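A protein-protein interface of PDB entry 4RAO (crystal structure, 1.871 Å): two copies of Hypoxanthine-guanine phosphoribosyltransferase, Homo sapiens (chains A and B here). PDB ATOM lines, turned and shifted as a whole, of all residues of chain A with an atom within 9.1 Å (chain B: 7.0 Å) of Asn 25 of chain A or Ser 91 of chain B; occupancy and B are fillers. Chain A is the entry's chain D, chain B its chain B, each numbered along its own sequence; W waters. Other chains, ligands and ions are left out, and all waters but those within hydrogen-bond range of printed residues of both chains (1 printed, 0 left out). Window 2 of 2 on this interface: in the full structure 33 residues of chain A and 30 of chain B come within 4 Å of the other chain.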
ATOM      1  N   PHE A  21      27.422  -7.516  25.546  1.00  0.00           N
ATOM      2  CA  PHE A  21      27.410  -6.157  25.039  1.00  0.00           C
ATOM      3  C   PHE A  21      26.489  -5.239  25.835  1.00  0.00           C
ATOM      4  O   PHE A  21      25.712  -5.691  26.675  1.00  0.00           O
ATOM      5  CB  PHE A  21      27.001  -6.167  23.568  1.00  0.00           C
ATOM      6  CG  PHE A  21      27.988  -6.850  22.682  1.00  0.00           C
ATOM      7  CD1 PHE A  21      29.021  -6.134  22.104  1.00  0.00           C
ATOM      8  CD2 PHE A  21      27.898  -8.212  22.436  1.00  0.00           C
ATOM      9  CE1 PHE A  21      29.957  -6.765  21.288  1.00  0.00           C
ATOM     10  CE2 PHE A  21      28.825  -8.849  21.625  1.00  0.00           C
ATOM     11  CZ  PHE A  21      29.854  -8.123  21.045  1.00  0.00           C
ATOM     12  N   CYS A  22      26.605  -3.937  25.581  1.00  0.00           N
ATOM     13  CA  CYS A  22      25.704  -2.964  26.179  1.00  0.00           C
ATOM     14  C   CYS A  22      24.505  -2.853  25.251  1.00  0.00           C
ATOM     15  O   CYS A  22      24.653  -2.483  24.090  1.00  0.00           O
ATOM     16  CB  CYS A  22      26.390  -1.613  26.327  1.00  0.00           C
ATOM     17  N   ILE A  23      23.320  -3.177  25.768  1.00  0.00           N
ATOM     18  CA  ILE A  23      22.089  -3.215  24.970  1.00  0.00           C
ATOM     19  C   ILE A  23      21.043  -2.315  25.627  1.00  0.00           C
ATOM     20  O   ILE A  23      20.946  -2.292  26.848  1.00  0.00           O
ATOM     21  CB  ILE A  23      21.531  -4.669  24.911  1.00  0.00           C
ATOM     22  CG1 ILE A  23      22.556  -5.622  24.280  1.00  0.00           C
ATOM     23  CG2 ILE A  23      20.196  -4.735  24.169  1.00  0.00           C
ATOM     24  CD1 ILE A  23      22.952  -5.261  22.853  1.00  0.00           C
ATOM     25  N   PRO A  24      20.260  -1.571  24.825  1.00  0.00           N
ATOM     26  CA  PRO A  24      19.212  -0.754  25.456  1.00  0.00           C
ATOM     27  C   PRO A  24      18.215  -1.620  26.212  1.00  0.00           C
ATOM     28  O   PRO A  24      17.724  -2.609  25.664  1.00  0.00           O
ATOM     29  CB  PRO A  24      18.533  -0.050  24.268  1.00  0.00           C
ATOM     30  CG  PRO A  24      19.005  -0.754  23.034  1.00  0.00           C
ATOM     31  CD  PRO A  24      20.348  -1.352  23.372  1.00  0.00           C
ATOM     32  N   ASN A  25      17.942  -1.258  27.466  1.00  0.00           N
ATOM     33  CA  ASN A  25      17.072  -2.040  28.334  1.00  0.00           C
ATOM     34  C   ASN A  25      15.703  -2.329  27.742  1.00  0.00           C
ATOM     35  O   ASN A  25      15.115  -3.383  27.995  1.00  0.00           O
ATOM     36  CB  ASN A  25      16.874  -1.322  29.674  1.00  0.00           C
ATOM     37  CG  ASN A  25      18.182  -1.051  30.395  1.00  0.00           C
ATOM     38  OD1 ASN A  25      18.894  -0.097  30.071  1.00  0.00           O
ATOM     39  ND2 ASN A  25      18.499  -1.881  31.384  1.00  0.00           N
ATOM     40  N   HIS A  26      15.179  -1.382  26.975  1.00  0.00           N
ATOM     41  CA  HIS A  26      13.816  -1.514  26.481  1.00  0.00           C
ATOM     42  C   HIS A  26      13.690  -2.533  25.342  1.00  0.00           C
ATOM     43  O   HIS A  26      12.583  -2.944  24.994  1.00  0.00           O
ATOM     44  CB  HIS A  26      13.246  -0.146  26.082  1.00  0.00           C
ATOM     45  CG  HIS A  26      14.011   0.541  24.992  1.00  0.00           C
ATOM     46  ND1 HIS A  26      15.090   1.364  25.238  1.00  0.00           N
ATOM     47  CD2 HIS A  26      13.837   0.541  23.648  1.00  0.00           C
ATOM     48  CE1 HIS A  26      15.552   1.834  24.092  1.00  0.00           C
ATOM     49  NE2 HIS A  26      14.809   1.353  23.113  1.00  0.00           N
ATOM     50  N   TYR A  27      14.826  -2.937  24.773  1.00  0.00           N
ATOM     51  CA  TYR A  27      14.844  -3.971  23.742  1.00  0.00           C
ATOM     52  C   TYR A  27      15.382  -5.306  24.271  1.00  0.00           C
ATOM     53  O   TYR A  27      15.506  -6.265  23.512  1.00  0.00           O
ATOM     54  CB  TYR A  27      15.673  -3.523  22.527  1.00  0.00           C
ATOM     55  CG  TYR A  27      15.037  -2.417  21.717  1.00  0.00           C
ATOM     56  CD1 TYR A  27      13.658  -2.352  21.547  1.00  0.00           C
ATOM     57  CD2 TYR A  27      15.818  -1.440  21.124  1.00  0.00           C
ATOM     58  CE1 TYR A  27      13.084  -1.342  20.799  1.00  0.00           C
ATOM     59  CE2 TYR A  27      15.257  -0.431  20.388  1.00  0.00           C
ATOM     60  CZ  TYR A  27      13.894  -0.384  20.233  1.00  0.00           C
ATOM     61  OH  TYR A  27      13.350   0.631  19.495  1.00  0.00           O
ATOM     62  N   ALA A  28      15.675  -5.363  25.570  1.00  0.00           N
ATOM     63  CA  ALA A  28      16.317  -6.532  26.196  1.00  0.00           C
ATOM     64  C   ALA A  28      15.790  -7.913  25.776  1.00  0.00           C
ATOM     65  O   ALA A  28      16.558  -8.756  25.322  1.00  0.00           O
ATOM     66  CB  ALA A  28      16.300  -6.403  27.715  1.00  0.00           C
ATOM     67  N   GLU A  29      14.493  -8.155  25.936  1.00  0.00           N
ATOM     68  CA  GLU A  29      13.941  -9.459  25.566  1.00  0.00           C
ATOM     69  C   GLU A  29      13.298  -9.475  24.180  1.00  0.00           C
ATOM     70  O   GLU A  29      12.603 -10.423  23.817  1.00  0.00           O
ATOM     71  CB  GLU A  29      12.972  -9.988  26.631  1.00  0.00           C
ATOM     72  CG  GLU A  29      13.678 -10.543  27.870  1.00  0.00           C
ATOM     73  CD  GLU A  29      12.938 -11.705  28.519  1.00  0.00           C
ATOM     74  OE1 GLU A  29      11.688 -11.687  28.549  1.00  0.00           O
ATOM     75  OE2 GLU A  29      13.610 -12.643  29.000  1.00  0.00           O
ATOM     76  N   ASP A  30      13.550  -8.428  23.401  1.00  0.00           N
ATOM     77  CA  ASP A  30      12.979  -8.312  22.064  1.00  0.00           C
ATOM     78  C   ASP A  30      13.990  -8.751  21.011  1.00  0.00           C
ATOM     79  O   ASP A  30      13.659  -8.894  19.832  1.00  0.00           O
ATOM     80  CB  ASP A  30      12.548  -6.862  21.791  1.00  0.00           C
ATOM     81  CG  ASP A  30      11.423  -6.398  22.711  1.00  0.00           C
ATOM     82  OD1 ASP A  30      10.532  -7.216  23.036  1.00  0.00           O
ATOM     83  OD2 ASP A  30      11.436  -5.210  23.109  1.00  0.00           O
ATOM     84  N   LEU A  31      15.232  -8.951  21.439  1.00  0.00           N
ATOM     85  CA  LEU A  31      16.296  -9.337  20.521  1.00  0.00           C
ATOM     86  C   LEU A  31      16.769 -10.734  20.892  1.00  0.00           C
ATOM     87  O   LEU A  31      16.557 -11.185  22.017  1.00  0.00           O
ATOM     88  CB  LEU A  31      17.450  -8.346  20.597  1.00  0.00           C
ATOM     89  CG  LEU A  31      17.114  -6.897  20.231  1.00  0.00           C
ATOM     90  CD1 LEU A  31      18.259  -5.970  20.606  1.00  0.00           C
ATOM     91  CD2 LEU A  31      16.807  -6.788  18.749  1.00  0.00           C
ATOM     92  N   ASP A 200      16.712   2.780  16.971  1.00  0.00           N
ATOM     93  CA  ASP A 200      17.504   3.379  18.048  1.00  0.00           C
ATOM     94  C   ASP A 200      18.362   2.324  18.749  1.00  0.00           C
ATOM     95  O   ASP A 200      18.267   2.119  19.958  1.00  0.00           O
ATOM     96  CB  ASP A 200      16.591   4.074  19.070  1.00  0.00           C
ATOM     97  CG  ASP A 200      15.481   3.162  19.578  1.00  0.00           C
ATOM     98  OD1 ASP A 200      14.982   2.348  18.775  1.00  0.00           O
ATOM     99  OD2 ASP A 200      15.113   3.255  20.776  1.00  0.00           O
ATOM    100  N   LEU A 201      19.192   1.649  17.967  1.00  0.00           N
ATOM    101  CA  LEU A 201      20.017   0.544  18.445  1.00  0.00           C
ATOM    102  C   LEU A 201      21.259   0.600  17.590  1.00  0.00           C
ATOM    103  O   LEU A 201      21.146   0.722  16.372  1.00  0.00           O
ATOM    104  CB  LEU A 201      19.271  -0.776  18.251  1.00  0.00           C
ATOM    105  CG  LEU A 201      19.982  -2.105  18.455  1.00  0.00           C
ATOM    106  CD1 LEU A 201      20.438  -2.241  19.899  1.00  0.00           C
ATOM    107  CD2 LEU A 201      19.034  -3.244  18.086  1.00  0.00           C
ATOM    108  N   LYS A 214       5.459  -8.469  19.689  1.00  0.00           N
ATOM    109  CA  LYS A 214       5.248  -7.249  20.452  1.00  0.00           C
ATOM    110  C   LYS A 214       5.085  -6.046  19.533  1.00  0.00           C
ATOM    111  O   LYS A 214       4.270  -5.157  19.794  1.00  0.00           O
ATOM    112  CB  LYS A 214       6.462  -7.047  21.356  1.00  0.00           C
ATOM    113  CG  LYS A 214       6.346  -6.032  22.477  1.00  0.00           C
ATOM    114  CD  LYS A 214       7.489  -6.291  23.453  1.00  0.00           C
ATOM    115  CE  LYS A 214       7.714  -5.169  24.442  1.00  0.00           C
ATOM    116  NZ  LYS A 214       8.957  -5.427  25.231  1.00  0.00           N
ATOM    117  N   TYR A 215       5.864  -6.025  18.454  1.00  0.00           N
ATOM    118  CA  TYR A 215       5.904  -4.869  17.565  1.00  0.00           C
ATOM    119  C   TYR A 215       5.150  -5.076  16.254  1.00  0.00           C
ATOM    120  O   TYR A 215       5.034  -4.156  15.449  1.00  0.00           O
ATOM    121  CB  TYR A 215       7.354  -4.438  17.326  1.00  0.00           C
ATOM    122  CG  TYR A 215       8.025  -4.002  18.608  1.00  0.00           C
ATOM    123  CD1 TYR A 215       7.581  -2.874  19.288  1.00  0.00           C
ATOM    124  CD2 TYR A 215       9.078  -4.730  19.156  1.00  0.00           C
ATOM    125  CE1 TYR A 215       8.167  -2.470  20.471  1.00  0.00           C
ATOM    126  CE2 TYR A 215       9.681  -4.331  20.342  1.00  0.00           C
ATOM    127  CZ  TYR A 215       9.216  -3.200  20.995  1.00  0.00           C
ATOM    128  OH  TYR A 215       9.792  -2.791  22.174  1.00  0.00           O
ATOM    129  N   MET B  53      16.899  13.494  28.161  1.00  0.00           N
ATOM    130  CA  MET B  53      16.421  12.331  28.906  1.00  0.00           C
ATOM    131  C   MET B  53      15.908  12.684  30.303  1.00  0.00           C
ATOM    132  O   MET B  53      14.992  12.036  30.810  1.00  0.00           O
ATOM    133  CB  MET B  53      17.475  11.219  28.944  1.00  0.00           C
ATOM    134  CG  MET B  53      17.691  10.544  27.589  1.00  0.00           C
ATOM    135  SD  MET B  53      16.184   9.860  26.843  1.00  0.00           S
ATOM    136  CE  MET B  53      15.913   8.413  27.855  1.00  0.00           C
ATOM    137  N   MET B  56      12.372  14.265  29.026  1.00  0.00           N
ATOM    138  CA  MET B  56      11.458  13.520  28.153  1.00  0.00           C
ATOM    139  C   MET B  56      11.435  11.999  28.303  1.00  0.00           C
ATOM    140  O   MET B  56      10.634  11.325  27.651  1.00  0.00           O
ATOM    141  CB  MET B  56      11.742  13.852  26.686  1.00  0.00           C
ATOM    142  CG  MET B  56      11.809  15.325  26.375  1.00  0.00           C
ATOM    143  SD  MET B  56      11.991  15.561  24.611  1.00  0.00           S
ATOM    144  CE  MET B  56      10.366  15.049  24.035  1.00  0.00           C
ATOM    145  N   GLY B  57      12.310  11.454  29.139  1.00  0.00           N
ATOM    146  CA  GLY B  57      12.342  10.018  29.359  1.00  0.00           C
ATOM    147  C   GLY B  57      11.999   9.651  30.791  1.00  0.00           C
ATOM    148  O   GLY B  57      12.551  10.226  31.732  1.00  0.00           O
ATOM    149  N   GLY B  58      11.121   8.667  30.962  1.00  0.00           N
ATOM    150  CA  GLY B  58      10.676   7.855  29.847  1.00  0.00           C
ATOM    151  C   GLY B  58       9.188   7.692  29.579  1.00  0.00           C
ATOM    152  O   GLY B  58       8.471   6.981  30.296  1.00  0.00           O
ATOM    153  N   HIS B  59       8.728   8.394  28.546  1.00  0.00           N
ATOM    154  CA  HIS B  59       7.670   7.902  27.688  1.00  0.00           C
ATOM    155  C   HIS B  59       8.378   7.709  26.349  1.00  0.00           C
ATOM    156  O   HIS B  59       9.535   8.099  26.198  1.00  0.00           O
ATOM    157  CB  HIS B  59       6.512   8.894  27.555  1.00  0.00           C
ATOM    158  CG  HIS B  59       5.356   8.368  26.756  1.00  0.00           C
ATOM    159  ND1 HIS B  59       4.949   7.050  26.816  1.00  0.00           N
ATOM    160  CD2 HIS B  59       4.526   8.975  25.875  1.00  0.00           C
ATOM    161  CE1 HIS B  59       3.918   6.871  26.008  1.00  0.00           C
ATOM    162  NE2 HIS B  59       3.639   8.023  25.428  1.00  0.00           N
ATOM    163  N   HIS B  60       7.704   7.086  25.395  1.00  0.00           N
ATOM    164  CA  HIS B  60       8.236   6.921  24.055  1.00  0.00           C
ATOM    165  C   HIS B  60       8.453   8.300  23.431  1.00  0.00           C
ATOM    166  O   HIS B  60       7.596   9.174  23.548  1.00  0.00           O
ATOM    167  CB  HIS B  60       7.227   6.117  23.230  1.00  0.00           C
ATOM    168  CG  HIS B  60       7.657   5.857  21.823  1.00  0.00           C
ATOM    169  ND1 HIS B  60       7.818   6.861  20.892  1.00  0.00           N
ATOM    170  CD2 HIS B  60       7.948   4.699  21.179  1.00  0.00           C
ATOM    171  CE1 HIS B  60       8.202   6.337  19.743  1.00  0.00           C
ATOM    172  NE2 HIS B  60       8.288   5.030  19.890  1.00  0.00           N
ATOM    173  N   ILE B  61       9.593   8.472  22.756  1.00  0.00           N
ATOM    174  CA  ILE B  61       9.946   9.714  22.070  1.00  0.00           C
ATOM    175  C   ILE B  61       9.955   9.510  20.556  1.00  0.00           C
ATOM    176  O   ILE B  61      10.524   8.529  20.070  1.00  0.00           O
ATOM    177  CB  ILE B  61      11.358  10.204  22.493  1.00  0.00           C
ATOM    178  CG1 ILE B  61      11.364  10.643  23.959  1.00  0.00           C
ATOM    179  CG2 ILE B  61      11.827  11.352  21.620  1.00  0.00           C
ATOM    180  CD1 ILE B  61      12.759  10.808  24.542  1.00  0.00           C
ATOM    181  N   ILE B  81      22.008  10.033  23.085  1.00  0.00           N
ATOM    182  CA  ILE B  81      20.839   9.497  23.798  1.00  0.00           C
ATOM    183  C   ILE B  81      20.876   7.961  23.819  1.00  0.00           C
ATOM    184  O   ILE B  81      20.612   7.337  24.837  1.00  0.00           O
ATOM    185  CB  ILE B  81      19.502   9.987  23.188  1.00  0.00           C
ATOM    186  CG1 ILE B  81      19.316  11.482  23.447  1.00  0.00           C
ATOM    187  CG2 ILE B  81      18.318   9.231  23.799  1.00  0.00           C
ATOM    188  CD1 ILE B  81      18.265  12.135  22.538  1.00  0.00           C
ATOM    189  N   LEU B  84      23.168   6.691  26.522  1.00  0.00           N
ATOM    190  CA  LEU B  84      22.535   6.732  27.836  1.00  0.00           C
ATOM    191  C   LEU B  84      21.560   5.563  27.996  1.00  0.00           C
ATOM    192  O   LEU B  84      21.463   4.960  29.077  1.00  0.00           O
ATOM    193  CB  LEU B  84      21.775   8.055  28.016  1.00  0.00           C
ATOM    194  CG  LEU B  84      22.562   9.355  28.038  1.00  0.00           C
ATOM    195  CD1 LEU B  84      21.627  10.583  28.020  1.00  0.00           C
ATOM    196  CD2 LEU B  84      23.455   9.391  29.279  1.00  0.00           C
ATOM    197  N   ASN B  85      20.822   5.260  26.929  1.00  0.00           N
ATOM    198  CA  ASN B  85      19.821   4.187  26.979  1.00  0.00           C
ATOM    199  C   ASN B  85      20.406   2.804  27.235  1.00  0.00           C
ATOM    200  O   ASN B  85      19.714   1.923  27.736  1.00  0.00           O
ATOM    201  CB  ASN B  85      19.001   4.144  25.683  1.00  0.00           C
ATOM    202  CG  ASN B  85      17.947   5.214  25.625  1.00  0.00           C
ATOM    203  OD1 ASN B  85      17.492   5.703  26.651  1.00  0.00           O
ATOM    204  ND2 ASN B  85      17.539   5.573  24.419  1.00  0.00           N
ATOM    205  N   ARG B  86      21.671   2.601  26.882  1.00  0.00           N
ATOM    206  CA  ARG B  86      22.276   1.276  27.069  1.00  0.00           C
ATOM    207  C   ARG B  86      23.264   1.207  28.238  1.00  0.00           C
ATOM    208  O   ARG B  86      23.690   0.119  28.636  1.00  0.00           O
ATOM    209  CB  ARG B  86      22.919   0.770  25.768  1.00  0.00           C
ATOM    210  CG  ARG B  86      24.139   1.557  25.337  1.00  0.00           C
ATOM    211  CD  ARG B  86      24.692   1.103  23.996  1.00  0.00           C
ATOM    212  NE  ARG B  86      25.818   1.964  23.645  1.00  0.00           N
ATOM    213  CZ  ARG B  86      25.810   2.896  22.698  1.00  0.00           C
ATOM    214  NH1 ARG B  86      24.735   3.093  21.937  1.00  0.00           N
ATOM    215  NH2 ARG B  86      26.898   3.634  22.511  1.00  0.00           N
ATOM    216  N   ASN B  87      23.600   2.362  28.810  1.00  0.00           N
ATOM    217  CA  ASN B  87      24.560   2.407  29.917  1.00  0.00           C
ATOM    218  C   ASN B  87      24.001   2.909  31.248  1.00  0.00           C
ATOM    219  O   ASN B  87      24.577   2.641  32.310  1.00  0.00           O
ATOM    220  CB  ASN B  87      25.790   3.235  29.525  1.00  0.00           C
ATOM    221  CG  ASN B  87      26.706   2.498  28.559  1.00  0.00           C
ATOM    222  OD1 ASN B  87      27.098   1.355  28.813  1.00  0.00           O
ATOM    223  ND2 ASN B  87      27.040   3.146  27.445  1.00  0.00           N
ATOM    224  N   SER B  88      22.884   3.628  31.206  1.00  0.00           N
ATOM    225  CA  SER B  88      22.366   4.227  32.438  1.00  0.00           C
ATOM    226  C   SER B  88      21.119   3.554  33.011  1.00  0.00           C
ATOM    227  O   SER B  88      20.775   2.421  32.661  1.00  0.00           O
ATOM    228  CB  SER B  88      22.119   5.732  32.266  1.00  0.00           C
ATOM    229  OG  SER B  88      20.954   5.977  31.502  1.00  0.00           O
ATOM    230  N   ASP B  89      20.452   4.291  33.893  1.00  0.00           N
ATOM    231  CA  ASP B  89      19.361   3.780  34.709  1.00  0.00           C
ATOM    232  C   ASP B  89      17.990   4.179  34.168  1.00  0.00           C
ATOM    233  O   ASP B  89      16.987   4.078  34.873  1.00  0.00           O
ATOM    234  CB  ASP B  89      19.514   4.313  36.134  1.00  0.00           C
ATOM    235  CG  ASP B  89      19.719   5.821  36.171  1.00  0.00           C
ATOM    236  OD1 ASP B  89      19.141   6.486  37.058  1.00  0.00           O
ATOM    237  OD2 ASP B  89      20.459   6.342  35.306  1.00  0.00           O
ATOM    238  N   ARG B  90      17.949   4.640  32.923  1.00  0.00           N
ATOM    239  CA  ARG B  90      16.694   5.077  32.316  1.00  0.00           C
ATOM    240  C   ARG B  90      16.684   4.757  30.833  1.00  0.00           C
ATOM    241  O   ARG B  90      17.739   4.562  30.231  1.00  0.00           O
ATOM    242  CB  ARG B  90      16.485   6.566  32.540  1.00  0.00           C
ATOM    243  N   SER B  91      15.496   4.713  30.241  1.00  0.00           N
ATOM    244  CA  SER B  91      15.376   4.363  28.829  1.00  0.00           C
ATOM    245  C   SER B  91      14.452   5.266  28.019  1.00  0.00           C
ATOM    246  O   SER B  91      13.550   5.911  28.562  1.00  0.00           O
ATOM    247  CB  SER B  91      14.909   2.913  28.677  1.00  0.00           C
ATOM    248  OG  SER B  91      15.999   2.047  28.408  1.00  0.00           O
ATOM    249  N   ILE B  92      14.697   5.299  26.712  1.00  0.00           N
ATOM    250  CA  ILE B  92      13.721   5.772  25.737  1.00  0.00           C
ATOM    251  C   ILE B  92      12.613   4.677  25.667  1.00  0.00           C
ATOM    252  O   ILE B  92      12.043   4.384  26.713  1.00  0.00           O
ATOM    253  CB  ILE B  92      14.401   6.069  24.439  1.00  0.00           C
ATOM    254  N   PRO B  93      12.290   4.036  24.511  1.00  0.00           N
ATOM    255  CA  PRO B  93      12.539   3.865  23.070  1.00  0.00           C
ATOM    256  C   PRO B  93      12.279   5.126  22.282  1.00  0.00           C
ATOM    257  O   PRO B  93      11.537   6.004  22.731  1.00  0.00           O
ATOM    258  CB  PRO B  93      11.503   2.812  22.652  1.00  0.00           C
ATOM    259  CG  PRO B  93      10.446   2.912  23.663  1.00  0.00           C
ATOM    260  CD  PRO B  93      11.208   3.127  24.929  1.00  0.00           C
HETATM  261  O   HOH W   1      18.371   3.060  22.377  1.00  0.00           O
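Of the 18 printed residues of chain B, 5 touch a printed residue of chain A. Hydrophobic or aromatic side chains of chain B within 4 Å of the printed part of chain A: Pro 93. Printed residues of chain A that touch a printed residue of chain B: Cys 22, Ile 23, Pro 24, Asn 25, His 26 and Asp 200.
OD1 of Asn 25 of chain A sits close to O of Asn 85 of chain B (3.2 Å). The side-chain hydroxyl (OG) of Ser 91 of chain B lies within hydrogen-bond range of a ring nitrogen (ND1) of His 26 of chain A (3.4 Å).
Cys 22 of chain A touches Arg 86 of chain B (O to CD, 3.6 Å). Cys 22 of chain A touches Asn 87 of chain B. Ile 23 of chain A touches Arg 86 of chain B (C to CB, 3.6 Å). CA of Pro 24 of chain A touches O of Asn 85 of chain B, 3.6 Å away. Pro 24 of chain A touches Arg 86 of chain B. Ser 91 of chain B touches Asn 25 of chain A. His 26 of chain A touches Pro 93 of chain B (NE2 to CA, 3.4 Å). Pro 93 of chain B touches Asp 200 of chain A.
Printed residues of chain B within 4 Å of Ile 23 of chain A: Arg 86. Asn 25 of chain A touches two residues of chain B. Printed residues of chain B within 4 Å of His 26 of chain A: Ser 91 (3.4 Å) and Pro 93 (3.4 Å). Leu 201 of chain A touches none of the printed residues of chain B. Gly 57 of chain B touches none of the printed residues of chain A. No residue of chain A comes within 4 Å of Arg 90 of chain B. Ser 91 of chain B touches two residues of chain A. Ile 92 of chain B touches none of the printed residues of chain A. Of the printed residues of chain A, Pro 93 of chain B touches His 26 and Asp 200. The nearest residue of chain A that does not touch Ser 91 of chain B is Pro 24 of chain A (4.8 Å). The nearest printed residue of chain B that does not touch Asp 200 of chain A is Ile 92 of chain B (4.7 Å).
No position is printed for both chains.
Water W1 bridges O of Asp 200 of chain A (2.6 Å) and ND2 of Asn 85 of chain B (3.3 Å).
The backbone NH of Ile 61 of chain B lies within hydrogen-bond range of the backbone carbonyl oxygen of Pro 93 of chain B. OD1 of Asn 85 of chain B sits at hydrogen-bond distance from N of Ile 92 of chain B, at 2.8 Å. A ring nitrogen (NE2) of His 26 of chain A lies within hydrogen-bond range of the side-chain carboxylate (OD2) of Asp 200 of chain A, 3.0 Å away. The side-chain hydroxyl (OH) of Tyr 27 of chain A is in hydrogen-bond range of the side-chain carboxylate (OD1) of Asp 200 of chain A (2.5 Å).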
